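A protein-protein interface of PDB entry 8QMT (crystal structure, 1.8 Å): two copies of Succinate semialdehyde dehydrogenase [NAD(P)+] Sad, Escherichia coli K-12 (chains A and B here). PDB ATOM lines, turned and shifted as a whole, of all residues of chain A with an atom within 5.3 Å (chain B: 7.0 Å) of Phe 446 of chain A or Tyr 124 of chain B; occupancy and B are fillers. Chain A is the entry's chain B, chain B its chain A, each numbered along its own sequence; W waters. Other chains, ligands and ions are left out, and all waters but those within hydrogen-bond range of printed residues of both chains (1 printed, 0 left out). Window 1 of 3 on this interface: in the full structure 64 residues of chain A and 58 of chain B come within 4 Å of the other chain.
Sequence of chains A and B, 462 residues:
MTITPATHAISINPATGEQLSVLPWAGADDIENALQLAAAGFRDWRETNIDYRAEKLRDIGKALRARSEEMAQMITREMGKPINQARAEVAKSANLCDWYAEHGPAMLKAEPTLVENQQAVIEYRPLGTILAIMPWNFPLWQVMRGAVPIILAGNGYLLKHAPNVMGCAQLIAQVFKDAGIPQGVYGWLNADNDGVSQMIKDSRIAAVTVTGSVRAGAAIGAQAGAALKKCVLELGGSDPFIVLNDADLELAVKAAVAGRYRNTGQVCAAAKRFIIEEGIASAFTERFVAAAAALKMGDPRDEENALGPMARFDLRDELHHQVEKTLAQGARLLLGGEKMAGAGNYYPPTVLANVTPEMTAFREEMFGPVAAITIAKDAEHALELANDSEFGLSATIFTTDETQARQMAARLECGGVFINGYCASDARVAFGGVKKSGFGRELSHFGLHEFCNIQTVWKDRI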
ATOM      1  N   VAL A 429       4.066  37.285 -17.751  1.00  0.00           N
ATOM      2  CA  VAL A 429       3.544  36.065 -18.358  1.00  0.00           C
ATOM      3  C   VAL A 429       4.399  34.879 -17.922  1.00  0.00           C
ATOM      4  O   VAL A 429       5.560  35.028 -17.543  1.00  0.00           O
ATOM      5  CB  VAL A 429       3.501  36.155 -19.907  1.00  0.00           C
ATOM      6  CG1 VAL A 429       2.809  37.437 -20.371  1.00  0.00           C
ATOM      7  CG2 VAL A 429       4.903  36.080 -20.503  1.00  0.00           C
ATOM      8  N   ALA A 430       3.816  33.681 -18.007  1.00  0.00           N
ATOM      9  CA  ALA A 430       4.532  32.485 -17.582  1.00  0.00           C
ATOM     10  C   ALA A 430       5.680  32.163 -18.533  1.00  0.00           C
ATOM     11  O   ALA A 430       5.634  32.461 -19.733  1.00  0.00           O
ATOM     12  CB  ALA A 430       3.582  31.290 -17.494  1.00  0.00           C
ATOM     13  N   ARG A 441       7.096  26.527 -13.918  1.00  0.00           N
ATOM     14  CA  ARG A 441       6.915  27.806 -14.592  1.00  0.00           C
ATOM     15  C   ARG A 441       7.563  28.916 -13.785  1.00  0.00           C
ATOM     16  O   ARG A 441       7.573  28.874 -12.554  1.00  0.00           O
ATOM     17  CB  ARG A 441       5.423  28.108 -14.817  1.00  0.00           C
ATOM     18  CG  ARG A 441       4.743  27.160 -15.816  1.00  0.00           C
ATOM     19  CD  ARG A 441       5.317  27.366 -17.229  1.00  0.00           C
ATOM     20  NE  ARG A 441       4.728  26.464 -18.214  1.00  0.00           N
ATOM     21  CZ  ARG A 441       5.269  25.310 -18.584  1.00  0.00           C
ATOM     22  NH1 ARG A 441       6.359  24.843 -17.999  1.00  0.00           N
ATOM     23  NH2 ARG A 441       4.713  24.618 -19.581  1.00  0.00           N
ATOM     24  N   GLU A 442       8.126  29.899 -14.488  1.00  0.00           N
ATOM     25  CA  GLU A 442       8.742  31.047 -13.852  1.00  0.00           C
ATOM     26  C   GLU A 442       7.977  32.310 -14.227  1.00  0.00           C
ATOM     27  O   GLU A 442       7.150  32.314 -15.141  1.00  0.00           O
ATOM     28  CB  GLU A 442      10.225  31.138 -14.236  1.00  0.00           C
ATOM     29  CG  GLU A 442      10.986  29.910 -13.731  1.00  0.00           C
ATOM     30  CD  GLU A 442      12.492  30.096 -13.616  1.00  0.00           C
ATOM     31  OE1 GLU A 442      12.947  31.127 -13.062  1.00  0.00           O
ATOM     32  OE2 GLU A 442      13.220  29.187 -14.078  1.00  0.00           O
ATOM     33  N   LEU A 443       8.239  33.372 -13.460  1.00  0.00           N
ATOM     34  CA  LEU A 443       7.695  34.711 -13.681  1.00  0.00           C
ATOM     35  C   LEU A 443       6.195  34.763 -13.403  1.00  0.00           C
ATOM     36  O   LEU A 443       5.580  33.738 -13.070  1.00  0.00           O
ATOM     37  CB  LEU A 443       8.044  35.198 -15.099  1.00  0.00           C
ATOM     38  CG  LEU A 443       9.564  35.312 -15.284  1.00  0.00           C
ATOM     39  CD1 LEU A 443       9.957  35.749 -16.715  1.00  0.00           C
ATOM     40  CD2 LEU A 443      10.158  36.276 -14.260  1.00  0.00           C
ATOM     41  N   SER A 444       5.620  35.960 -13.477  1.00  0.00           N
ATOM     42  CA  SER A 444       4.234  36.255 -13.079  1.00  0.00           C
ATOM     43  C   SER A 444       4.011  35.684 -11.675  1.00  0.00           C
ATOM     44  O   SER A 444       4.936  35.664 -10.854  1.00  0.00           O
ATOM     45  CB  SER A 444       3.254  35.753 -14.137  1.00  0.00           C
ATOM     46  OG  SER A 444       1.926  36.159 -13.815  1.00  0.00           O
ATOM     47  N   HIS A 445       2.790  35.224 -11.382  1.00  0.00           N
ATOM     48  CA  HIS A 445       2.555  34.604 -10.081  1.00  0.00           C
ATOM     49  C   HIS A 445       3.081  33.177 -10.008  1.00  0.00           C
ATOM     50  O   HIS A 445       3.245  32.647  -8.900  1.00  0.00           O
ATOM     51  CB  HIS A 445       1.062  34.641  -9.712  1.00  0.00           C
ATOM     52  CG  HIS A 445       0.149  34.071 -10.757  1.00  0.00           C
ATOM     53  ND1 HIS A 445      -0.118  32.723 -10.862  1.00  0.00           N
ATOM     54  CD2 HIS A 445      -0.585  34.674 -11.722  1.00  0.00           C
ATOM     55  CE1 HIS A 445      -0.959  32.518 -11.861  1.00  0.00           C
ATOM     56  NE2 HIS A 445      -1.254  33.686 -12.403  1.00  0.00           N
ATOM     57  N   PHE A 446       3.383  32.560 -11.154  1.00  0.00           N
ATOM     58  CA  PHE A 446       3.877  31.185 -11.161  1.00  0.00           C
ATOM     59  C   PHE A 446       5.247  31.087 -10.503  1.00  0.00           C
ATOM     60  O   PHE A 446       5.480  30.213  -9.660  1.00  0.00           O
ATOM     61  CB  PHE A 446       3.924  30.658 -12.596  1.00  0.00           C
ATOM     62  CG  PHE A 446       2.665  30.932 -13.372  1.00  0.00           C
ATOM     63  CD1 PHE A 446       1.572  30.083 -13.269  1.00  0.00           C
ATOM     64  CD2 PHE A 446       2.574  32.052 -14.190  1.00  0.00           C
ATOM     65  CE1 PHE A 446       0.406  30.342 -13.971  1.00  0.00           C
ATOM     66  CE2 PHE A 446       1.415  32.318 -14.896  1.00  0.00           C
ATOM     67  CZ  PHE A 446       0.328  31.458 -14.785  1.00  0.00           C
ATOM     68  N   GLY A 447       6.167  31.986 -10.863  1.00  0.00           N
ATOM     69  CA  GLY A 447       7.482  31.960 -10.249  1.00  0.00           C
ATOM     70  C   GLY A 447       7.455  32.249  -8.759  1.00  0.00           C
ATOM     71  O   GLY A 447       8.360  31.836  -8.027  1.00  0.00           O
ATOM     72  N   LEU A 448       6.443  32.990  -8.295  1.00  0.00           N
ATOM     73  CA  LEU A 448       6.252  33.196  -6.861  1.00  0.00           C
ATOM     74  C   LEU A 448       5.802  31.911  -6.185  1.00  0.00           C
ATOM     75  O   LEU A 448       6.325  31.519  -5.132  1.00  0.00           O
ATOM     76  CB  LEU A 448       5.201  34.279  -6.614  1.00  0.00           C
ATOM     77  CG  LEU A 448       5.506  35.707  -6.176  1.00  0.00           C
ATOM     78  CD1 LEU A 448       4.203  36.358  -5.729  1.00  0.00           C
ATOM     79  CD2 LEU A 448       6.548  35.769  -5.070  1.00  0.00           C
ATOM     80  N   HIS A 449       4.813  31.249  -6.767  1.00  0.00           N
ATOM     81  CA  HIS A 449       4.123  30.172  -6.076  1.00  0.00           C
ATOM     82  C   HIS A 449       4.833  28.831  -6.178  1.00  0.00           C
ATOM     83  O   HIS A 449       4.567  27.947  -5.355  1.00  0.00           O
ATOM     84  CB  HIS A 449       2.701  30.053  -6.632  1.00  0.00           C
ATOM     85  CG  HIS A 449       1.828  31.219  -6.291  1.00  0.00           C
ATOM     86  ND1 HIS A 449       0.627  31.465  -6.923  1.00  0.00           N
ATOM     87  CD2 HIS A 449       1.978  32.200  -5.371  1.00  0.00           C
ATOM     88  CE1 HIS A 449       0.072  32.545  -6.402  1.00  0.00           C
ATOM     89  NE2 HIS A 449       0.868  33.007  -5.453  1.00  0.00           N
ATOM     90  N   GLU A 450       5.725  28.653  -7.163  1.00  0.00           N
ATOM     91  CA  GLU A 450       6.364  27.353  -7.339  1.00  0.00           C
ATOM     92  C   GLU A 450       7.115  26.919  -6.092  1.00  0.00           C
ATOM     93  O   GLU A 450       7.187  25.721  -5.802  1.00  0.00           O
ATOM     94  CB  GLU A 450       7.323  27.376  -8.529  1.00  0.00           C
ATOM     95  CG  GLU A 450       6.629  27.326  -9.866  1.00  0.00           C
ATOM     96  CD  GLU A 450       6.313  25.917 -10.327  1.00  0.00           C
ATOM     97  OE1 GLU A 450       6.436  24.953  -9.540  1.00  0.00           O
ATOM     98  OE2 GLU A 450       5.933  25.777 -11.498  1.00  0.00           O
ATOM     99  N   ARG B  53     -16.574  17.224 -21.177  1.00  0.00           N
ATOM    100  CA  ARG B  53     -15.861  16.476 -20.143  1.00  0.00           C
ATOM    101  C   ARG B  53     -16.536  16.614 -18.789  1.00  0.00           C
ATOM    102  O   ARG B  53     -16.566  15.659 -18.002  1.00  0.00           O
ATOM    103  CB  ARG B  53     -14.413  16.940 -20.074  1.00  0.00           C
ATOM    104  CG  ARG B  53     -13.743  16.811 -21.412  1.00  0.00           C
ATOM    105  CD  ARG B  53     -12.265  16.706 -21.260  1.00  0.00           C
ATOM    106  NE  ARG B  53     -11.650  17.937 -20.790  1.00  0.00           N
ATOM    107  CZ  ARG B  53     -11.006  18.796 -21.568  1.00  0.00           C
ATOM    108  NH1 ARG B  53     -10.999  18.670 -22.883  1.00  0.00           N
ATOM    109  NH2 ARG B  53     -10.341  19.798 -21.009  1.00  0.00           N
ATOM    110  N   MET B 107     -12.209  26.995 -13.514  1.00  0.00           N
ATOM    111  CA  MET B 107     -10.797  27.023 -13.141  1.00  0.00           C
ATOM    112  C   MET B 107      -9.861  26.805 -14.324  1.00  0.00           C
ATOM    113  O   MET B 107      -8.652  27.039 -14.191  1.00  0.00           O
ATOM    114  CB  MET B 107     -10.522  25.964 -12.076  1.00  0.00           C
ATOM    115  CG  MET B 107     -11.278  26.180 -10.787  1.00  0.00           C
ATOM    116  SD  MET B 107     -11.154  24.746  -9.693  1.00  0.00           S
ATOM    117  CE  MET B 107     -11.828  25.449  -8.199  1.00  0.00           C
ATOM    118  N   LEU B 108     -10.374  26.371 -15.473  1.00  0.00           N
ATOM    119  CA  LEU B 108      -9.538  26.107 -16.632  1.00  0.00           C
ATOM    120  C   LEU B 108      -9.651  27.190 -17.696  1.00  0.00           C
ATOM    121  O   LEU B 108      -9.072  27.047 -18.780  1.00  0.00           O
ATOM    122  CB  LEU B 108      -9.880  24.741 -17.220  1.00  0.00           C
ATOM    123  CG  LEU B 108      -9.414  23.580 -16.337  1.00  0.00           C
ATOM    124  CD1 LEU B 108      -9.962  22.264 -16.866  1.00  0.00           C
ATOM    125  CD2 LEU B 108      -7.889  23.555 -16.276  1.00  0.00           C
ATOM    126  N   LYS B 109     -10.379  28.266 -17.412  1.00  0.00           N
ATOM    127  CA  LYS B 109     -10.478  29.367 -18.357  1.00  0.00           C
ATOM    128  C   LYS B 109      -9.149  30.115 -18.447  1.00  0.00           C
ATOM    129  O   LYS B 109      -8.347  30.127 -17.511  1.00  0.00           O
ATOM    130  CB  LYS B 109     -11.606  30.319 -17.951  1.00  0.00           C
ATOM    131  CG  LYS B 109     -12.998  29.677 -18.003  1.00  0.00           C
ATOM    132  CD  LYS B 109     -13.393  29.321 -19.440  1.00  0.00           C
ATOM    133  CE  LYS B 109     -14.182  28.007 -19.523  1.00  0.00           C
ATOM    134  NZ  LYS B 109     -13.347  26.809 -19.157  1.00  0.00           N
ATOM    135  N   ALA B 110      -8.916  30.728 -19.599  1.00  0.00           N
ATOM    136  CA  ALA B 110      -7.668  31.447 -19.819  1.00  0.00           C
ATOM    137  C   ALA B 110      -7.540  32.625 -18.862  1.00  0.00           C
ATOM    138  O   ALA B 110      -8.530  33.278 -18.521  1.00  0.00           O
ATOM    139  CB  ALA B 110      -7.602  31.931 -21.265  1.00  0.00           C
ATOM    140  N   GLU B 111      -6.303  32.898 -18.419  1.00  0.00           N
ATOM    141  CA  GLU B 111      -6.065  34.056 -17.559  1.00  0.00           C
ATOM    142  C   GLU B 111      -5.724  35.276 -18.402  1.00  0.00           C
ATOM    143  O   GLU B 111      -4.908  35.179 -19.319  1.00  0.00           O
ATOM    144  CB  GLU B 111      -4.897  33.820 -16.606  1.00  0.00           C
ATOM    145  CG  GLU B 111      -5.142  32.927 -15.451  1.00  0.00           C
ATOM    146  CD  GLU B 111      -3.905  32.800 -14.577  1.00  0.00           C
ATOM    147  OE1 GLU B 111      -3.077  33.739 -14.546  1.00  0.00           O
ATOM    148  OE2 GLU B 111      -3.754  31.759 -13.917  1.00  0.00           O
ATOM    149  N   ILE B 122      -2.849  33.454 -20.522  1.00  0.00           N
ATOM    150  CA  ILE B 122      -2.315  32.184 -20.055  1.00  0.00           C
ATOM    151  C   ILE B 122      -3.392  31.135 -20.280  1.00  0.00           C
ATOM    152  O   ILE B 122      -4.521  31.287 -19.797  1.00  0.00           O
ATOM    153  CB  ILE B 122      -1.924  32.223 -18.571  1.00  0.00           C
ATOM    154  CG1 ILE B 122      -1.038  33.439 -18.243  1.00  0.00           C
ATOM    155  CG2 ILE B 122      -1.250  30.921 -18.208  1.00  0.00           C
ATOM    156  CD1 ILE B 122       0.239  33.551 -19.089  1.00  0.00           C
ATOM    157  N   GLU B 123      -3.048  30.078 -21.009  1.00  0.00           N
ATOM    158  CA  GLU B 123      -3.961  28.978 -21.291  1.00  0.00           C
ATOM    159  C   GLU B 123      -3.539  27.752 -20.494  1.00  0.00           C
ATOM    160  O   GLU B 123      -2.347  27.497 -20.321  1.00  0.00           O
ATOM    161  CB  GLU B 123      -3.965  28.631 -22.784  1.00  0.00           C
ATOM    162  CG  GLU B 123      -4.446  29.745 -23.692  1.00  0.00           C
ATOM    163  CD  GLU B 123      -5.955  29.783 -23.851  1.00  0.00           C
ATOM    164  OE1 GLU B 123      -6.658  29.004 -23.179  1.00  0.00           O
ATOM    165  OE2 GLU B 123      -6.442  30.596 -24.668  1.00  0.00           O
ATOM    166  N   TYR B 124      -4.520  26.977 -20.031  1.00  0.00           N
ATOM    167  CA  TYR B 124      -4.258  25.745 -19.286  1.00  0.00           C
ATOM    168  C   TYR B 124      -4.487  24.570 -20.232  1.00  0.00           C
ATOM    169  O   TYR B 124      -5.624  24.149 -20.446  1.00  0.00           O
ATOM    170  CB  TYR B 124      -5.148  25.670 -18.046  1.00  0.00           C
ATOM    171  CG  TYR B 124      -4.702  26.637 -16.994  1.00  0.00           C
ATOM    172  CD1 TYR B 124      -3.694  26.293 -16.096  1.00  0.00           C
ATOM    173  CD2 TYR B 124      -5.236  27.918 -16.928  1.00  0.00           C
ATOM    174  CE1 TYR B 124      -3.252  27.184 -15.136  1.00  0.00           C
ATOM    175  CE2 TYR B 124      -4.797  28.818 -15.973  1.00  0.00           C
ATOM    176  CZ  TYR B 124      -3.806  28.445 -15.078  1.00  0.00           C
ATOM    177  OH  TYR B 124      -3.368  29.344 -14.128  1.00  0.00           O
ATOM    178  N   ARG B 125      -3.411  24.063 -20.810  1.00  0.00           N
ATOM    179  CA  ARG B 125      -3.468  22.970 -21.772  1.00  0.00           C
ATOM    180  C   ARG B 125      -3.175  21.653 -21.072  1.00  0.00           C
ATOM    181  O   ARG B 125      -2.435  21.630 -20.089  1.00  0.00           O
ATOM    182  CB  ARG B 125      -2.434  23.151 -22.891  1.00  0.00           C
ATOM    183  CG  ARG B 125      -2.335  24.542 -23.517  1.00  0.00           C
ATOM    184  CD  ARG B 125      -3.568  24.934 -24.316  1.00  0.00           C
ATOM    185  NE  ARG B 125      -3.232  26.050 -25.208  1.00  0.00           N
ATOM    186  CZ  ARG B 125      -4.105  26.736 -25.933  1.00  0.00           C
ATOM    187  NH1 ARG B 125      -5.399  26.446 -25.910  1.00  0.00           N
ATOM    188  NH2 ARG B 125      -3.666  27.736 -26.703  1.00  0.00           N
ATOM    189  N   PRO B 126      -3.692  20.525 -21.552  1.00  0.00           N
ATOM    190  CA  PRO B 126      -3.275  19.246 -20.971  1.00  0.00           C
ATOM    191  C   PRO B 126      -1.823  18.940 -21.313  1.00  0.00           C
ATOM    192  O   PRO B 126      -1.264  19.438 -22.301  1.00  0.00           O
ATOM    193  CB  PRO B 126      -4.232  18.228 -21.606  1.00  0.00           C
ATOM    194  CG  PRO B 126      -4.678  18.866 -22.879  1.00  0.00           C
ATOM    195  CD  PRO B 126      -4.674  20.355 -22.640  1.00  0.00           C
ATOM    196  N   ALA B 153      -9.006  18.195 -17.013  1.00  0.00           N
ATOM    197  CA  ALA B 153      -8.075  19.105 -17.687  1.00  0.00           C
ATOM    198  C   ALA B 153      -7.678  18.632 -19.083  1.00  0.00           C
ATOM    199  O   ALA B 153      -6.913  19.321 -19.768  1.00  0.00           O
ATOM    200  CB  ALA B 153      -6.826  19.295 -16.812  1.00  0.00           C
ATOM    201  N   HIS B 445      -8.342  23.974  -7.315  1.00  0.00           N
ATOM    202  CA  HIS B 445      -7.731  24.235  -8.617  1.00  0.00           C
ATOM    203  C   HIS B 445      -6.308  23.697  -8.705  1.00  0.00           C
ATOM    204  O   HIS B 445      -5.788  23.523  -9.813  1.00  0.00           O
ATOM    205  CB  HIS B 445      -7.756  25.739  -8.942  1.00  0.00           C
ATOM    206  CG  HIS B 445      -7.167  26.618  -7.876  1.00  0.00           C
ATOM    207  ND1 HIS B 445      -5.829  26.940  -7.830  1.00  0.00           N
ATOM    208  CD2 HIS B 445      -7.742  27.260  -6.830  1.00  0.00           C
ATOM    209  CE1 HIS B 445      -5.602  27.735  -6.800  1.00  0.00           C
ATOM    210  NE2 HIS B 445      -6.746  27.948  -6.179  1.00  0.00           N
ATOM    211  N   LEU B 448      -6.135  20.407 -10.534  1.00  0.00           N
ATOM    212  CA  LEU B 448      -6.377  20.575 -11.960  1.00  0.00           C
ATOM    213  C   LEU B 448      -5.137  21.098 -12.677  1.00  0.00           C
ATOM    214  O   LEU B 448      -4.848  20.693 -13.808  1.00  0.00           O
ATOM    215  CB  LEU B 448      -7.538  21.542 -12.189  1.00  0.00           C
ATOM    216  CG  LEU B 448      -8.996  21.136 -12.075  1.00  0.00           C
ATOM    217  CD1 LEU B 448      -9.820  22.402 -12.196  1.00  0.00           C
ATOM    218  CD2 LEU B 448      -9.363  20.136 -13.175  1.00  0.00           C
ATOM    219  N   HIS B 449      -4.391  21.998 -12.036  1.00  0.00           N
ATOM    220  CA  HIS B 449      -3.314  22.702 -12.732  1.00  0.00           C
ATOM    221  C   HIS B 449      -1.956  22.016 -12.630  1.00  0.00           C
ATOM    222  O   HIS B 449      -1.082  22.298 -13.460  1.00  0.00           O
ATOM    223  CB  HIS B 449      -3.186  24.133 -12.201  1.00  0.00           C
ATOM    224  CG  HIS B 449      -4.363  25.003 -12.519  1.00  0.00           C
ATOM    225  ND1 HIS B 449      -4.585  26.209 -11.892  1.00  0.00           N
ATOM    226  CD2 HIS B 449      -5.376  24.847 -13.404  1.00  0.00           C
ATOM    227  CE1 HIS B 449      -5.695  26.750 -12.361  1.00  0.00           C
ATOM    228  NE2 HIS B 449      -6.192  25.946 -13.283  1.00  0.00           N
ATOM    229  N   CYS B 452      -1.084  20.488 -15.959  1.00  0.00           N
ATOM    230  CA  CYS B 452      -1.318  21.278 -17.157  1.00  0.00           C
ATOM    231  C   CYS B 452      -0.012  21.834 -17.700  1.00  0.00           C
ATOM    232  O   CYS B 452       0.933  22.118 -16.956  1.00  0.00           O
ATOM    233  CB  CYS B 452      -2.275  22.442 -16.894  1.00  0.00           C
ATOM    234  SG  CYS B 452      -4.026  21.933 -16.772  1.00  0.00           S
ATOM    235  N   ASN B 453       0.023  21.964 -19.019  1.00  0.00           N
ATOM    236  CA  ASN B 453       0.982  22.826 -19.695  1.00  0.00           C
ATOM    237  C   ASN B 453       0.447  24.244 -19.563  1.00  0.00           C
ATOM    238  O   ASN B 453      -0.500  24.625 -20.250  1.00  0.00           O
ATOM    239  CB  ASN B 453       1.135  22.410 -21.155  1.00  0.00           C
ATOM    240  CG  ASN B 453       1.876  23.444 -21.982  1.00  0.00           C
ATOM    241  OD1 ASN B 453       2.530  24.337 -21.444  1.00  0.00           O
ATOM    242  ND2 ASN B 453       1.784  23.317 -23.303  1.00  0.00           N
ATOM    243  N   ILE B 454       1.032  25.020 -18.655  1.00  0.00           N
ATOM    244  CA  ILE B 454       0.642  26.410 -18.467  1.00  0.00           C
ATOM    245  C   ILE B 454       1.302  27.210 -19.589  1.00  0.00           C
ATOM    246  O   ILE B 454       2.525  27.362 -19.614  1.00  0.00           O
ATOM    247  CB  ILE B 454       1.047  26.919 -17.080  1.00  0.00           C
ATOM    248  CG1 ILE B 454       0.147  26.267 -16.012  1.00  0.00           C
ATOM    249  CG2 ILE B 454       0.954  28.429 -17.001  1.00  0.00           C
ATOM    250  CD1 ILE B 454       0.446  26.726 -14.619  1.00  0.00           C
ATOM    251  N   GLN B 455       0.497  27.687 -20.538  1.00  0.00           N
ATOM    252  CA  GLN B 455       1.009  28.151 -21.828  1.00  0.00           C
ATOM    253  C   GLN B 455       0.719  29.628 -22.033  1.00  0.00           C
ATOM    254  O   GLN B 455      -0.444  30.041 -22.040  1.00  0.00           O
ATOM    255  CB  GLN B 455       0.391  27.340 -22.963  1.00  0.00           C
ATOM    256  CG  GLN B 455       1.018  27.586 -24.331  1.00  0.00           C
ATOM    257  CD  GLN B 455       0.226  26.907 -25.434  1.00  0.00           C
ATOM    258  OE1 GLN B 455      -0.970  27.145 -25.575  1.00  0.00           O
ATOM    259  NE2 GLN B 455       0.884  26.047 -26.209  1.00  0.00           N
ATOM    260  N   THR B 456       1.773  30.413 -22.254  1.00  0.00           N
ATOM    261  CA  THR B 456       1.607  31.801 -22.643  1.00  0.00           C
ATOM    262  C   THR B 456       1.321  31.845 -24.134  1.00  0.00           C
ATOM    263  O   THR B 456       2.026  31.205 -24.918  1.00  0.00           O
ATOM    264  CB  THR B 456       2.867  32.608 -22.319  1.00  0.00           C
ATOM    265  OG1 THR B 456       3.055  32.637 -20.899  1.00  0.00           O
ATOM    266  CG2 THR B 456       2.748  34.044 -22.859  1.00  0.00           C
HETATM  267  O   HOH W   1       4.997  29.058 -19.983  1.00  0.00           O
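Phe 446 of chain A touches just these residues of chain B: Ile 122 (3.8 Å), Tyr 124 (3.9 Å) and Ile 454 (3.6 Å). Of chain A, only Phe 446 (3.9 Å) comes within 4 Å of Tyr 124 of chain B. Printed residues of chain A within 4 Å of Glu 111 of chain B: His 445 (2.8 Å). Of the printed residues of chain A, Ile 454 of chain B touches Ala 430 (3.9 Å), Arg 441 (2.8 Å) and Phe 446 (3.6 Å). Printed residues of chain B within 4 Å of Val 429 of chain A: Thr 456. Gln 455 of chain B touches none of the printed residues of chain A. The nearest residue of chain A that does not touch Tyr 124 of chain B is His 445 of chain A (4.6 Å).
N of Glu 111 of chain B lies within hydrogen-bond range of O of Ile 122 of chain B, 2.8 Å away. OH of Tyr 124 of chain B sits at hydrogen-bond distance from OE2 of Glu 111 of chain B (2.5 Å). The backbone NH (N) of Asn 453 of chain B lies within hydrogen-bond range of the backbone carbonyl oxygen (O) of Arg 125 of chain B (2.7 Å). OE2 of Glu 450 of chain A lies within hydrogen-bond range of N of Arg 441 of chain A (2.8 Å). A ring nitrogen (ND1) of His 449 of chain A lies close to the backbone carbonyl oxygen (O) of His 445 of chain A (3.5 Å).
OE1 of Glu 111 of chain B lies within hydrogen-bond range of NE2 of His 445 of chain A (2.8 Å). OD1 of Asn 453 of chain B is in hydrogen-bond range of NH2 of Arg 441 of chain A, 2.9 Å away. The backbone carbonyl oxygen of Ile 454 of chain B sits at hydrogen-bond distance from the guanidinium group of Arg 441 of chain A (2.8 Å). O of Ala 430 of chain A lies within hydrogen-bond range of OG1 of Thr 456 of chain B, at 2.8 Å.
Water W1 lies within hydrogen-bond range of O of Ile 454 of chain B (3.0 Å), NE of Arg 441 of chain A (3.2 Å) and O of Ala 430 of chain A (3.5 Å).
Hydrophobic or aromatic side chains of chain A within 4 Å of the printed part of chain B: Val 429, Ala 430, His 445 and Phe 446. Along chain A the printed residues that touch a printed residue of chain B span positions 429 to 446. Printed residues of chain B that touch a printed residue of chain A: Glu 111, Ile 122, Tyr 124, Asn 453, Ile 454 and Thr 456. Hydrophobic or aromatic side chains of chain B that line the printed part of chain A: Ile 122, Tyr 124 and Ile 454. Among the printed residues, 10 pairs touch across the chains.
Among the printed residues, merely in contact across the chains: Phe 446 of chain A with Ile 454 of chain B, Val 429 of chain A with Thr 456 of chain B, Ala 430 of chain A with Ile 122 of chain B, Phe 446 of chain A with Ile 122 of chain B, Phe 446 of chain A with Tyr 124 of chain B and Ala 430 of chain A with Ile 454 of chain B.
Positions printed for both chains: 445, 448 and 449.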
